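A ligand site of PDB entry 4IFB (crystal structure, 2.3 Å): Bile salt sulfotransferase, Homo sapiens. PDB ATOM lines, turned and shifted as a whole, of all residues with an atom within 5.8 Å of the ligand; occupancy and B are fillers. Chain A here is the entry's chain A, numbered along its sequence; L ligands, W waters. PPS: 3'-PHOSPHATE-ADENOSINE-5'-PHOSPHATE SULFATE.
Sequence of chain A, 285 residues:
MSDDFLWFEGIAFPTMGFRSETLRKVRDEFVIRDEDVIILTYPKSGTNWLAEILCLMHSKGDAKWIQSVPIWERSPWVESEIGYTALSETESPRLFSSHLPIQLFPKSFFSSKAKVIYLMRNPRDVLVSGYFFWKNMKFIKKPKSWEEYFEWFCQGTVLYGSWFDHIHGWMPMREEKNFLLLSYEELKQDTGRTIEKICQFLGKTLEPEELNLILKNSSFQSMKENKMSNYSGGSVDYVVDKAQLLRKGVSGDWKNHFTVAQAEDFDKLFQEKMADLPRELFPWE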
ATOM      1  N   THR A  41     -23.235  -4.382 -20.385  1.00  0.00           N
ATOM      2  CA  THR A  41     -22.942  -3.330 -21.377  1.00  0.00           C
ATOM      3  C   THR A  41     -21.947  -2.391 -20.791  1.00  0.00           C
ATOM      4  O   THR A  41     -21.961  -2.127 -19.563  1.00  0.00           O
ATOM      5  CB  THR A  41     -24.185  -2.463 -21.710  1.00  0.00           C
ATOM      6  OG1 THR A  41     -24.663  -1.952 -20.477  1.00  0.00           O
ATOM      7  CG2 THR A  41     -25.267  -3.289 -22.319  1.00  0.00           C
ATOM      8  N   TYR A  42     -21.113  -1.837 -21.668  1.00  0.00           N
ATOM      9  CA  TYR A  42     -20.454  -0.584 -21.374  1.00  0.00           C
ATOM     10  C   TYR A  42     -21.535   0.515 -21.304  1.00  0.00           C
ATOM     11  O   TYR A  42     -22.467   0.486 -22.092  1.00  0.00           O
ATOM     12  CB  TYR A  42     -19.385  -0.303 -22.457  1.00  0.00           C
ATOM     13  CG  TYR A  42     -18.520   0.891 -22.154  1.00  0.00           C
ATOM     14  CD1 TYR A  42     -17.403   0.760 -21.327  1.00  0.00           C
ATOM     15  CD2 TYR A  42     -18.851   2.156 -22.626  1.00  0.00           C
ATOM     16  CE1 TYR A  42     -16.635   1.845 -21.015  1.00  0.00           C
ATOM     17  CE2 TYR A  42     -18.069   3.266 -22.329  1.00  0.00           C
ATOM     18  CZ  TYR A  42     -16.983   3.102 -21.510  1.00  0.00           C
ATOM     19  OH  TYR A  42     -16.204   4.189 -21.173  1.00  0.00           O
ATOM     20  N   PRO A  43     -21.452   1.460 -20.357  1.00  0.00           N
ATOM     21  CA  PRO A  43     -22.582   2.420 -20.235  1.00  0.00           C
ATOM     22  C   PRO A  43     -22.946   3.125 -21.522  1.00  0.00           C
ATOM     23  O   PRO A  43     -22.067   3.477 -22.282  1.00  0.00           O
ATOM     24  CB  PRO A  43     -22.111   3.437 -19.187  1.00  0.00           C
ATOM     25  CG  PRO A  43     -20.959   2.803 -18.491  1.00  0.00           C
ATOM     26  CD  PRO A  43     -20.374   1.733 -19.390  1.00  0.00           C
ATOM     27  N   LYS A  44     -24.251   3.337 -21.759  1.00  0.00           N
ATOM     28  CA  LYS A  44     -24.798   4.058 -22.907  1.00  0.00           C
ATOM     29  C   LYS A  44     -24.779   3.219 -24.196  1.00  0.00           C
ATOM     30  O   LYS A  44     -24.832   3.774 -25.313  1.00  0.00           O
ATOM     31  CB  LYS A  44     -24.092   5.397 -23.138  1.00  0.00           C
ATOM     32  CG  LYS A  44     -23.828   6.243 -21.884  1.00  0.00           C
ATOM     33  CD  LYS A  44     -25.014   6.361 -20.898  1.00  0.00           C
ATOM     34  CE  LYS A  44     -26.232   7.024 -21.491  1.00  0.00           C
ATOM     35  NZ  LYS A  44     -27.335   7.047 -20.457  1.00  0.00           N
ATOM     36  N   SER A  45     -24.732   1.902 -24.055  1.00  0.00           N
ATOM     37  CA  SER A  45     -24.750   1.031 -25.242  1.00  0.00           C
ATOM     38  C   SER A  45     -26.127   0.455 -25.541  1.00  0.00           C
ATOM     39  O   SER A  45     -26.280  -0.276 -26.518  1.00  0.00           O
ATOM     40  CB  SER A  45     -23.741  -0.113 -25.094  1.00  0.00           C
ATOM     41  OG  SER A  45     -22.445   0.390 -24.771  1.00  0.00           O
ATOM     42  N   GLY A  46     -27.114   0.750 -24.703  1.00  0.00           N
ATOM     43  CA  GLY A  46     -28.476   0.223 -24.935  1.00  0.00           C
ATOM     44  C   GLY A  46     -29.020  -0.669 -23.846  1.00  0.00           C
ATOM     45  O   GLY A  46     -29.926  -1.495 -24.084  1.00  0.00           O
ATOM     46  N   THR A  47     -28.499  -0.498 -22.631  1.00  0.00           N
ATOM     47  CA  THR A  47     -28.819  -1.413 -21.543  1.00  0.00           C
ATOM     48  C   THR A  47     -30.330  -1.444 -21.348  1.00  0.00           C
ATOM     49  O   THR A  47     -30.968  -2.512 -21.385  1.00  0.00           O
ATOM     50  CB  THR A  47     -28.195  -0.928 -20.220  1.00  0.00           C
ATOM     51  OG1 THR A  47     -26.870  -0.405 -20.441  1.00  0.00           O
ATOM     52  CG2 THR A  47     -28.201  -2.053 -19.168  1.00  0.00           C
ATOM     53  N   ASN A  48     -30.922  -0.263 -21.190  1.00  0.00           N
ATOM     54  CA  ASN A  48     -32.347  -0.156 -20.879  1.00  0.00           C
ATOM     55  C   ASN A  48     -33.271  -0.652 -21.966  1.00  0.00           C
ATOM     56  O   ASN A  48     -34.357  -1.183 -21.692  1.00  0.00           O
ATOM     57  CB  ASN A  48     -32.704   1.257 -20.441  1.00  0.00           C
ATOM     58  CG  ASN A  48     -32.101   1.578 -19.093  1.00  0.00           C
ATOM     59  OD1 ASN A  48     -32.639   1.168 -18.073  1.00  0.00           O
ATOM     60  ND2 ASN A  48     -30.910   2.217 -19.087  1.00  0.00           N
ATOM     61  N   TRP A  49     -32.783  -0.610 -23.182  1.00  0.00           N
ATOM     62  CA  TRP A  49     -33.581  -1.064 -24.287  1.00  0.00           C
ATOM     63  C   TRP A  49     -33.668  -2.582 -24.153  1.00  0.00           C
ATOM     64  O   TRP A  49     -34.712  -3.177 -24.285  1.00  0.00           O
ATOM     65  CB  TRP A  49     -32.890  -0.671 -25.601  1.00  0.00           C
ATOM     66  CG  TRP A  49     -33.668  -0.974 -26.884  1.00  0.00           C
ATOM     67  CD1 TRP A  49     -34.986  -1.303 -27.000  1.00  0.00           C
ATOM     68  CD2 TRP A  49     -33.170  -0.811 -28.234  1.00  0.00           C
ATOM     69  NE1 TRP A  49     -35.315  -1.448 -28.343  1.00  0.00           N
ATOM     70  CE2 TRP A  49     -34.223  -1.156 -29.107  1.00  0.00           C
ATOM     71  CE3 TRP A  49     -31.930  -0.459 -28.786  1.00  0.00           C
ATOM     72  CZ2 TRP A  49     -34.096  -1.096 -30.494  1.00  0.00           C
ATOM     73  CZ3 TRP A  49     -31.793  -0.427 -30.176  1.00  0.00           C
ATOM     74  CH2 TRP A  49     -32.883  -0.729 -31.012  1.00  0.00           C
ATOM     75  N   HIS A  99     -22.515  -3.001 -15.711  1.00  0.00           N
ATOM     76  CA  HIS A  99     -21.552  -2.399 -16.622  1.00  0.00           C
ATOM     77  C   HIS A  99     -20.086  -2.801 -16.303  1.00  0.00           C
ATOM     78  O   HIS A  99     -19.142  -2.289 -16.916  1.00  0.00           O
ATOM     79  CB  HIS A  99     -21.681  -0.861 -16.588  1.00  0.00           C
ATOM     80  CG  HIS A  99     -23.052  -0.345 -16.908  1.00  0.00           C
ATOM     81  ND1 HIS A  99     -23.734  -0.694 -18.052  1.00  0.00           N
ATOM     82  CD2 HIS A  99     -23.824   0.574 -16.274  1.00  0.00           C
ATOM     83  CE1 HIS A  99     -24.890  -0.023 -18.102  1.00  0.00           C
ATOM     84  NE2 HIS A  99     -24.954   0.762 -17.045  1.00  0.00           N
ATOM     85  N   ARG A 121     -22.003  -1.327 -28.686  1.00  0.00           N
ATOM     86  CA  ARG A 121     -22.437  -0.229 -29.520  1.00  0.00           C
ATOM     87  C   ARG A 121     -21.176   0.498 -29.988  1.00  0.00           C
ATOM     88  O   ARG A 121     -20.203   0.641 -29.223  1.00  0.00           O
ATOM     89  CB  ARG A 121     -23.267   0.756 -28.696  1.00  0.00           C
ATOM     90  CG  ARG A 121     -24.147   1.667 -29.523  1.00  0.00           C
ATOM     91  CD  ARG A 121     -24.832   2.737 -28.682  1.00  0.00           C
ATOM     92  NE  ARG A 121     -25.719   3.583 -29.501  1.00  0.00           N
ATOM     93  CZ  ARG A 121     -26.446   4.592 -29.022  1.00  0.00           C
ATOM     94  NH1 ARG A 121     -26.401   4.904 -27.730  1.00  0.00           N
ATOM     95  NH2 ARG A 121     -27.271   5.230 -29.818  1.00  0.00           N
ATOM     96  N   ASP A 125     -20.913   6.536 -30.951  1.00  0.00           N
ATOM     97  CA  ASP A 125     -22.297   6.794 -30.527  1.00  0.00           C
ATOM     98  C   ASP A 125     -22.441   6.734 -28.995  1.00  0.00           C
ATOM     99  O   ASP A 125     -23.168   7.530 -28.388  1.00  0.00           O
ATOM    100  CB  ASP A 125     -23.257   5.805 -31.233  1.00  0.00           C
ATOM    101  CG  ASP A 125     -23.433   6.121 -32.714  1.00  0.00           C
ATOM    102  OD1 ASP A 125     -23.218   7.283 -33.103  1.00  0.00           O
ATOM    103  OD2 ASP A 125     -23.795   5.218 -33.523  1.00  0.00           O
ATOM    104  N   VAL A 128     -21.201  10.121 -27.556  1.00  0.00           N
ATOM    105  CA  VAL A 128     -22.234  11.152 -27.703  1.00  0.00           C
ATOM    106  C   VAL A 128     -23.335  11.013 -26.652  1.00  0.00           C
ATOM    107  O   VAL A 128     -23.706  11.987 -25.953  1.00  0.00           O
ATOM    108  CB  VAL A 128     -22.840  11.127 -29.113  1.00  0.00           C
ATOM    109  CG1 VAL A 128     -24.002  12.116 -29.218  1.00  0.00           C
ATOM    110  CG2 VAL A 128     -21.763  11.472 -30.142  1.00  0.00           C
ATOM    111  N   SER A 129     -23.843   9.781 -26.558  1.00  0.00           N
ATOM    112  CA  SER A 129     -24.901   9.430 -25.622  1.00  0.00           C
ATOM    113  C   SER A 129     -24.540   9.795 -24.204  1.00  0.00           C
ATOM    114  O   SER A 129     -25.318  10.441 -23.514  1.00  0.00           O
ATOM    115  CB  SER A 129     -25.196   7.928 -25.740  1.00  0.00           C
ATOM    116  OG  SER A 129     -26.382   7.630 -25.029  1.00  0.00           O
ATOM    117  N   GLY A 130     -23.361   9.370 -23.740  1.00  0.00           N
ATOM    118  CA  GLY A 130     -22.961   9.675 -22.358  1.00  0.00           C
ATOM    119  C   GLY A 130     -22.709  11.156 -22.159  1.00  0.00           C
ATOM    120  O   GLY A 130     -23.056  11.713 -21.107  1.00  0.00           O
ATOM    121  N   PHE A 133     -26.123  12.720 -21.592  1.00  0.00           N
ATOM    122  CA  PHE A 133     -26.796  12.234 -20.395  1.00  0.00           C
ATOM    123  C   PHE A 133     -26.176  12.735 -19.111  1.00  0.00           C
ATOM    124  O   PHE A 133     -26.885  13.159 -18.198  1.00  0.00           O
ATOM    125  CB  PHE A 133     -26.771  10.715 -20.364  1.00  0.00           C
ATOM    126  CG  PHE A 133     -27.640  10.137 -19.302  1.00  0.00           C
ATOM    127  CD1 PHE A 133     -29.015  10.150 -19.436  1.00  0.00           C
ATOM    128  CD2 PHE A 133     -27.082   9.543 -18.181  1.00  0.00           C
ATOM    129  CE1 PHE A 133     -29.817   9.589 -18.473  1.00  0.00           C
ATOM    130  CE2 PHE A 133     -27.873   8.966 -17.228  1.00  0.00           C
ATOM    131  CZ  PHE A 133     -29.248   8.991 -17.371  1.00  0.00           C
ATOM    132  N   TRP A 134     -24.850  12.669 -19.060  1.00  0.00           N
ATOM    133  CA  TRP A 134     -24.075  12.953 -17.851  1.00  0.00           C
ATOM    134  C   TRP A 134     -23.627  14.391 -17.694  1.00  0.00           C
ATOM    135  O   TRP A 134     -23.047  14.757 -16.669  1.00  0.00           O
ATOM    136  CB  TRP A 134     -22.826  12.048 -17.826  1.00  0.00           C
ATOM    137  CG  TRP A 134     -23.150  10.635 -17.553  1.00  0.00           C
ATOM    138  CD1 TRP A 134     -24.083  10.186 -16.672  1.00  0.00           C
ATOM    139  CD2 TRP A 134     -22.564   9.470 -18.148  1.00  0.00           C
ATOM    140  NE1 TRP A 134     -24.118   8.806 -16.676  1.00  0.00           N
ATOM    141  CE2 TRP A 134     -23.200   8.341 -17.567  1.00  0.00           C
ATOM    142  CE3 TRP A 134     -21.555   9.264 -19.070  1.00  0.00           C
ATOM    143  CZ2 TRP A 134     -22.847   7.051 -17.895  1.00  0.00           C
ATOM    144  CZ3 TRP A 134     -21.210   7.967 -19.393  1.00  0.00           C
ATOM    145  CH2 TRP A 134     -21.844   6.874 -18.800  1.00  0.00           C
ATOM    146  N   TYR A 184     -25.907  -3.038 -30.696  1.00  0.00           N
ATOM    147  CA  TYR A 184     -26.980  -2.091 -30.790  1.00  0.00           C
ATOM    148  C   TYR A 184     -27.380  -1.828 -32.266  1.00  0.00           C
ATOM    149  O   TYR A 184     -28.567  -1.681 -32.596  1.00  0.00           O
ATOM    150  CB  TYR A 184     -26.530  -0.803 -30.102  1.00  0.00           C
ATOM    151  CG  TYR A 184     -27.528   0.338 -30.170  1.00  0.00           C
ATOM    152  CD1 TYR A 184     -28.226   0.742 -29.030  1.00  0.00           C
ATOM    153  CD2 TYR A 184     -27.703   1.088 -31.339  1.00  0.00           C
ATOM    154  CE1 TYR A 184     -29.097   1.821 -29.078  1.00  0.00           C
ATOM    155  CE2 TYR A 184     -28.598   2.141 -31.399  1.00  0.00           C
ATOM    156  CZ  TYR A 184     -29.306   2.492 -30.259  1.00  0.00           C
ATOM    157  OH  TYR A 184     -30.203   3.551 -30.311  1.00  0.00           O
ATOM    158  N   LYS A 188     -31.051  -2.258 -33.688  1.00  0.00           N
ATOM    159  CA  LYS A 188     -31.766  -1.140 -34.281  1.00  0.00           C
ATOM    160  C   LYS A 188     -32.218  -1.445 -35.710  1.00  0.00           C
ATOM    161  O   LYS A 188     -33.299  -1.044 -36.138  1.00  0.00           O
ATOM    162  CB  LYS A 188     -30.857   0.107 -34.269  1.00  0.00           C
ATOM    163  CG  LYS A 188     -31.450   1.324 -34.958  1.00  0.00           C
ATOM    164  CD  LYS A 188     -32.558   1.965 -34.143  1.00  0.00           C
ATOM    165  CE  LYS A 188     -33.269   3.039 -34.966  1.00  0.00           C
ATOM    166  NZ  LYS A 188     -34.317   3.693 -34.124  1.00  0.00           N
ATOM    167  N   SER A 218     -41.284  -1.996 -27.089  1.00  0.00           N
ATOM    168  CA  SER A 218     -39.884  -1.756 -26.857  1.00  0.00           C
ATOM    169  C   SER A 218     -39.289  -0.847 -27.960  1.00  0.00           C
ATOM    170  O   SER A 218     -38.074  -0.560 -27.960  1.00  0.00           O
ATOM    171  CB  SER A 218     -39.130  -3.091 -26.797  1.00  0.00           C
ATOM    172  OG  SER A 218     -39.101  -3.692 -28.081  1.00  0.00           O
ATOM    173  N   SER A 219     -40.116  -0.379 -28.884  1.00  0.00           N
ATOM    174  CA  SER A 219     -39.593   0.599 -29.877  1.00  0.00           C
ATOM    175  C   SER A 219     -39.327   1.949 -29.207  1.00  0.00           C
ATOM    176  O   SER A 219     -39.955   2.319 -28.202  1.00  0.00           O
ATOM    177  CB  SER A 219     -40.568   0.793 -31.044  1.00  0.00           C
ATOM    178  OG  SER A 219     -41.657   1.548 -30.544  1.00  0.00           O
ATOM    179  N   PHE A 220     -38.442   2.715 -29.802  1.00  0.00           N
ATOM    180  CA  PHE A 220     -38.047   4.002 -29.199  1.00  0.00           C
ATOM    181  C   PHE A 220     -39.244   4.883 -28.860  1.00  0.00           C
ATOM    182  O   PHE A 220     -39.383   5.330 -27.713  1.00  0.00           O
ATOM    183  CB  PHE A 220     -37.069   4.740 -30.116  1.00  0.00           C
ATOM    184  CG  PHE A 220     -36.542   6.029 -29.538  1.00  0.00           C
ATOM    185  CD1 PHE A 220     -35.473   6.022 -28.659  1.00  0.00           C
ATOM    186  CD2 PHE A 220     -37.137   7.250 -29.857  1.00  0.00           C
ATOM    187  CE1 PHE A 220     -34.992   7.207 -28.140  1.00  0.00           C
ATOM    188  CE2 PHE A 220     -36.641   8.442 -29.352  1.00  0.00           C
ATOM    189  CZ  PHE A 220     -35.569   8.423 -28.490  1.00  0.00           C
ATOM    190  N   MET A 223     -41.257   3.425 -25.741  1.00  0.00           N
ATOM    191  CA  MET A 223     -40.496   3.529 -24.492  1.00  0.00           C
ATOM    192  C   MET A 223     -40.352   4.956 -24.014  1.00  0.00           C
ATOM    193  O   MET A 223     -40.381   5.206 -22.817  1.00  0.00           O
ATOM    194  CB  MET A 223     -39.113   2.902 -24.640  1.00  0.00           C
ATOM    195  CG  MET A 223     -39.095   1.389 -24.614  1.00  0.00           C
ATOM    196  SD  MET A 223     -37.406   0.765 -24.453  1.00  0.00           S
ATOM    197  CE  MET A 223     -36.835   1.514 -22.931  1.00  0.00           C
ATOM    198  N   TYR A 231     -36.317   7.389 -17.551  1.00  0.00           N
ATOM    199  CA  TYR A 231     -36.014   8.324 -16.465  1.00  0.00           C
ATOM    200  C   TYR A 231     -34.950   9.338 -16.927  1.00  0.00           C
ATOM    201  O   TYR A 231     -34.661  10.319 -16.238  1.00  0.00           O
ATOM    202  CB  TYR A 231     -35.532   7.579 -15.226  1.00  0.00           C
ATOM    203  CG  TYR A 231     -34.307   6.743 -15.479  1.00  0.00           C
ATOM    204  CD1 TYR A 231     -33.058   7.350 -15.689  1.00  0.00           C
ATOM    205  CD2 TYR A 231     -34.383   5.352 -15.558  1.00  0.00           C
ATOM    206  CE1 TYR A 231     -31.933   6.585 -15.951  1.00  0.00           C
ATOM    207  CE2 TYR A 231     -33.262   4.574 -15.825  1.00  0.00           C
ATOM    208  CZ  TYR A 231     -32.039   5.202 -16.017  1.00  0.00           C
ATOM    209  OH  TYR A 231     -30.900   4.449 -16.285  1.00  0.00           O
ATOM    210  N   LEU A 245     -33.045   9.771 -20.717  1.00  0.00           N
ATOM    211  CA  LEU A 245     -32.413   8.510 -21.072  1.00  0.00           C
ATOM    212  C   LEU A 245     -32.634   8.160 -22.534  1.00  0.00           C
ATOM    213  O   LEU A 245     -31.700   7.722 -23.218  1.00  0.00           O
ATOM    214  CB  LEU A 245     -32.922   7.376 -20.176  1.00  0.00           C
ATOM    215  CG  LEU A 245     -32.309   5.992 -20.447  1.00  0.00           C
ATOM    216  CD1 LEU A 245     -30.934   5.828 -19.818  1.00  0.00           C
ATOM    217  CD2 LEU A 245     -33.281   4.918 -19.973  1.00  0.00           C
ATOM    218  N   LEU A 246     -33.848   8.348 -23.024  1.00  0.00           N
ATOM    219  CA  LEU A 246     -34.137   8.107 -24.441  1.00  0.00           C
ATOM    220  C   LEU A 246     -33.985   9.391 -25.241  1.00  0.00           C
ATOM    221  O   LEU A 246     -34.904  10.185 -25.345  1.00  0.00           O
ATOM    222  CB  LEU A 246     -35.515   7.463 -24.666  1.00  0.00           C
ATOM    223  CG  LEU A 246     -35.445   5.920 -24.683  1.00  0.00           C
ATOM    224  CD1 LEU A 246     -35.088   5.331 -23.331  1.00  0.00           C
ATOM    225  CD2 LEU A 246     -36.705   5.255 -25.219  1.00  0.00           C
ATOM    226  N   ARG A 247     -32.784   9.611 -25.769  1.00  0.00           N
ATOM    227  CA  ARG A 247     -32.467  10.916 -26.302  1.00  0.00           C
ATOM    228  C   ARG A 247     -32.838  10.990 -27.787  1.00  0.00           C
ATOM    229  O   ARG A 247     -33.483  11.920 -28.207  1.00  0.00           O
ATOM    230  CB  ARG A 247     -30.991  11.245 -26.068  1.00  0.00           C
ATOM    231  CG  ARG A 247     -30.539  12.605 -26.577  1.00  0.00           C
ATOM    232  CD  ARG A 247     -29.025  12.704 -26.569  1.00  0.00           C
ATOM    233  NE  ARG A 247     -28.399  11.617 -27.323  1.00  0.00           N
ATOM    234  CZ  ARG A 247     -27.932  11.732 -28.558  1.00  0.00           C
ATOM    235  NH1 ARG A 247     -27.998  12.884 -29.220  1.00  0.00           N
ATOM    236  NH2 ARG A 247     -27.393  10.667 -29.146  1.00  0.00           N
ATOM    237  N   LYS A 248     -32.435   9.990 -28.560  1.00  0.00           N
ATOM    238  CA  LYS A 248     -32.655  10.005 -29.997  1.00  0.00           C
ATOM    239  C   LYS A 248     -32.809   8.571 -30.510  1.00  0.00           C
ATOM    240  O   LYS A 248     -33.595   8.312 -31.416  1.00  0.00           O
ATOM    241  CB  LYS A 248     -31.449  10.671 -30.669  1.00  0.00           C
ATOM    242  CG  LYS A 248     -31.613  11.006 -32.149  1.00  0.00           C
ATOM    243  CD  LYS A 248     -30.418  11.854 -32.604  1.00  0.00           C
ATOM    244  CE  LYS A 248     -30.213  11.851 -34.104  1.00  0.00           C
ATOM    245  NZ  LYS A 248     -31.184  12.778 -34.724  1.00  0.00           N
ATOM    246  N   GLY A 249     -32.021   7.640 -29.974  1.00  0.00           N
ATOM    247  CA  GLY A 249     -32.241   6.242 -30.276  1.00  0.00           C
ATOM    248  C   GLY A 249     -31.915   5.817 -31.688  1.00  0.00           C
ATOM    249  O   GLY A 249     -32.593   4.931 -32.211  1.00  0.00           O
ATOM    250  N   VAL A 250     -30.864   6.375 -32.288  1.00  0.00           N
ATOM    251  CA  VAL A 250     -30.434   5.927 -33.650  1.00  0.00           C
ATOM    252  C   VAL A 250     -28.973   5.434 -33.616  1.00  0.00           C
ATOM    253  O   VAL A 250     -28.291   5.607 -32.607  1.00  0.00           O
ATOM    254  CB  VAL A 250     -30.620   7.049 -34.713  1.00  0.00           C
ATOM    255  CG1 VAL A 250     -32.098   7.470 -34.836  1.00  0.00           C
ATOM    256  CG2 VAL A 250     -29.769   8.265 -34.367  1.00  0.00           C
ATOM    257  N   ASP A 253     -25.508   8.916 -35.052  1.00  0.00           N
ATOM    258  CA  ASP A 253     -25.548  10.284 -34.531  1.00  0.00           C
ATOM    259  C   ASP A 253     -24.139  10.897 -34.240  1.00  0.00           C
ATOM    260  O   ASP A 253     -24.011  12.098 -34.064  1.00  0.00           O
ATOM    261  CB  ASP A 253     -26.385  10.361 -33.259  1.00  0.00           C
ATOM    262  CG  ASP A 253     -26.766  11.777 -32.927  1.00  0.00           C
ATOM    263  OD1 ASP A 253     -26.677  12.191 -31.736  1.00  0.00           O
ATOM    264  OD2 ASP A 253     -27.148  12.490 -33.899  1.00  0.00           O
HETATM  265  S2  PPS L   1     -27.311   3.494 -19.245  1.00  0.00           S
HETATM  266  OS1 PPS L   1     -27.641   4.693 -18.138  1.00  0.00           O
HETATM  267  OS2 PPS L   1     -25.885   3.200 -19.223  1.00  0.00           O
HETATM  268  OS3 PPS L   1     -28.029   2.308 -18.827  1.00  0.00           O
HETATM  269  O6P PPS L   1     -27.776   3.919 -20.688  1.00  0.00           O
HETATM  270  P2  PPS L   1     -28.154   2.814 -21.778  1.00  0.00           P
HETATM  271  O4P PPS L   1     -29.568   2.283 -21.457  1.00  0.00           O
HETATM  272  O5P PPS L   1     -27.141   1.701 -21.926  1.00  0.00           O
HETATM  273  O5' PPS L   1     -28.153   3.597 -23.185  1.00  0.00           O
HETATM  274  C5' PPS L   1     -29.007   4.680 -23.495  1.00  0.00           C
HETATM  275  C4' PPS L   1     -28.986   4.813 -25.018  1.00  0.00           C
HETATM  276  O4' PPS L   1     -29.782   3.768 -25.612  1.00  0.00           O
HETATM  277  C1' PPS L   1     -30.838   4.348 -26.338  1.00  0.00           C
HETATM  278  N9  PPS L   1     -32.106   3.602 -26.319  1.00  0.00           N
HETATM  279  C4  PPS L   1     -32.784   3.202 -27.401  1.00  0.00           C
HETATM  280  N3  PPS L   1     -32.546   3.181 -28.746  1.00  0.00           N
HETATM  281  C2  PPS L   1     -33.433   2.610 -29.599  1.00  0.00           C
HETATM  282  N1  PPS L   1     -34.616   2.094 -29.192  1.00  0.00           N
HETATM  283  C6  PPS L   1     -34.971   2.050 -27.886  1.00  0.00           C
HETATM  284  N6  PPS L   1     -36.167   1.520 -27.473  1.00  0.00           N
HETATM  285  C5  PPS L   1     -34.035   2.622 -26.900  1.00  0.00           C
HETATM  286  N7  PPS L   1     -34.029   2.768 -25.559  1.00  0.00           N
HETATM  287  C8  PPS L   1     -32.867   3.361 -25.215  1.00  0.00           C
HETATM  288  C2' PPS L   1     -31.035   5.718 -25.650  1.00  0.00           C
HETATM  289  O2' PPS L   1     -31.817   6.628 -26.457  1.00  0.00           O
HETATM  290  C3' PPS L   1     -29.585   6.143 -25.465  1.00  0.00           C
HETATM  291  O3' PPS L   1     -28.933   6.423 -26.718  1.00  0.00           O
HETATM  292  P1  PPS L   1     -28.828   7.887 -27.470  1.00  0.00           P
HETATM  293  O1P PPS L   1     -28.319   8.804 -26.355  1.00  0.00           O
HETATM  294  O2P PPS L   1     -30.249   8.176 -27.948  1.00  0.00           O
HETATM  295  O3P PPS L   1     -27.874   7.609 -28.588  1.00  0.00           O
HETATM  296  O   HOH W   1     -28.858   8.255 -31.077  1.00  0.00           O
HETATM  297  O   HOH W   2     -36.379   1.408 -31.220  1.00  0.00           O
HETATM  298  O   HOH W   3     -31.046   2.016 -23.554  1.00  0.00           O
HETATM  299  O   HOH W   4     -28.113  10.309 -24.039  1.00  0.00           O
HETATM  300  O   HOH W   5     -25.627   8.233 -29.942  1.00  0.00           O
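NE of Arg 247 lies within salt-bridge range of O1P of the ligand (3.0 Å). NH2 of Arg 121 lies within salt-bridge range of O3P of the ligand (2.7 Å). An oxygen (OS2) of the ligand lies within hydrogen-bond range of the backbone NH (N) of Lys 44 (3.0 Å). O of Leu 245 sits close to O2' of the ligand (3.4 Å). An oxygen (O4P) of the ligand is in hydrogen-bond range of the side-chain amide nitrogen (ND2) of Asn 48, 2.7 Å away. The side-chain hydroxyl (OG) of Ser 129 sits at hydrogen-bond distance from an oxygen (O1P) of the ligand. The side-chain hydroxyl (OG1) of Thr 47 sits at hydrogen-bond distance from an oxygen (O5P) of the ligand (2.6 Å). An oxygen (O5P) of the ligand lies within hydrogen-bond range of the backbone NH of Thr 47. The backbone NH (N) of Asn 48 is in hydrogen-bond range of an oxygen (O4P) of the ligand, at 2.9 Å. The backbone carbonyl oxygen of Ser 218 is in hydrogen-bond range of a nitrogen (N6) of the ligand, at 2.9 Å. A ring nitrogen (NE2) of His 99 is in hydrogen-bond range of an oxygen (OS2) of the ligand (3.4 Å). An oxygen (O2') of the ligand sits at hydrogen-bond distance from the backbone NH of Arg 247 (3.2 Å). The side-chain hydroxyl of Tyr 184 lies within hydrogen-bond range of a nitrogen (N3) of the ligand (2.8 Å). The backbone NH (N) of Gly 46 lies within hydrogen-bond range of an oxygen (O5P) of the ligand, at 2.9 Å. The backbone NH of Ser 45 sits at hydrogen-bond distance from an oxygen (O5P) of the ligand (3.2 Å). An oxygen (O2P) of the ligand is in hydrogen-bond range of the backbone NH (N) of Lys 248, at 2.9 Å. An oxygen (OS1) of the ligand is in salt-bridge range of the side-chain amino group of Lys 44 (3.3 Å). N6 of the ligand sits at hydrogen-bond distance from SD of Met 223, 3.4 Å away. N of Gly 249 lies within hydrogen-bond range of O2P of the ligand (2.7 Å).
N6 of the ligand lies close to NE1 of Trp 49 (3.2 Å). The backbone NH (N) of Phe 220 sits close to a nitrogen (N6) of the ligand, 3.5 Å away. Pro 43 touches the ligand. C of Ser 219 touches N6 of the ligand, at 3.6 Å. Tyr 231 touches the ligand. Leu 246 touches the ligand (CA to O2', 3.4 Å). 21 residues have an atom within 4 Å of the ligand: Pro 43, Lys 44, Ser 45, Gly 46, Thr 47, Asn 48, Trp 49, His 99, Arg 121, Ser 129, Tyr 184, Ser 218, Ser 219, Phe 220, Met 223, Tyr 231, Leu 245, Leu 246, Arg 247, Lys 248 and Gly 249.
Water W3 lies within hydrogen-bond range of an oxygen (O4P) of the ligand (2.6 Å), the backbone NH (N) of Trp 49 (3.2 Å) and the backbone NH (N) of Asn 48 (3.3 Å). Water W5 lies within hydrogen-bond range of an oxygen (O3P) of the ligand, the backbone carbonyl oxygen of Asp 125, the guanidinium group of Arg 247 and the guanidinium group of Arg 121. Water W4 bridges an oxygen (O1P) of the ligand (2.8 Å) and the backbone carbonyl oxygen of Ser 129 (2.8 Å). Water W2 lies within hydrogen-bond range of N1 of the ligand (2.8 Å) and N of Phe 220 (2.8 Å).
The side-chain hydroxyl (OG) of Ser 45 is in hydrogen-bond range of the backbone carbonyl oxygen (O) of Tyr 42, at 2.7 Å. O of Gly 249 is in hydrogen-bond range of NZ of Lys 188. The side-chain hydroxyl (OH) of Tyr 184 sits close to the backbone carbonyl oxygen (O) of Gly 249 (3.4 Å). NH1 of Arg 121 is in hydrogen-bond range of O of Lys 44, at 3.1 Å. The side-chain hydroxyl of Thr 41 sits at hydrogen-bond distance from the side-chain hydroxyl of Thr 47 (2.7 Å). The guanidinium group of Arg 247 is in salt-bridge range of the side-chain carboxylate of Asp 253 (2.9 Å). NH2 of Arg 121 is in hydrogen-bond range of O of Val 250. The backbone carbonyl oxygen (O) of Ser 218 sits at hydrogen-bond distance from the indole nitrogen (NE1) of Trp 49, 2.9 Å away.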
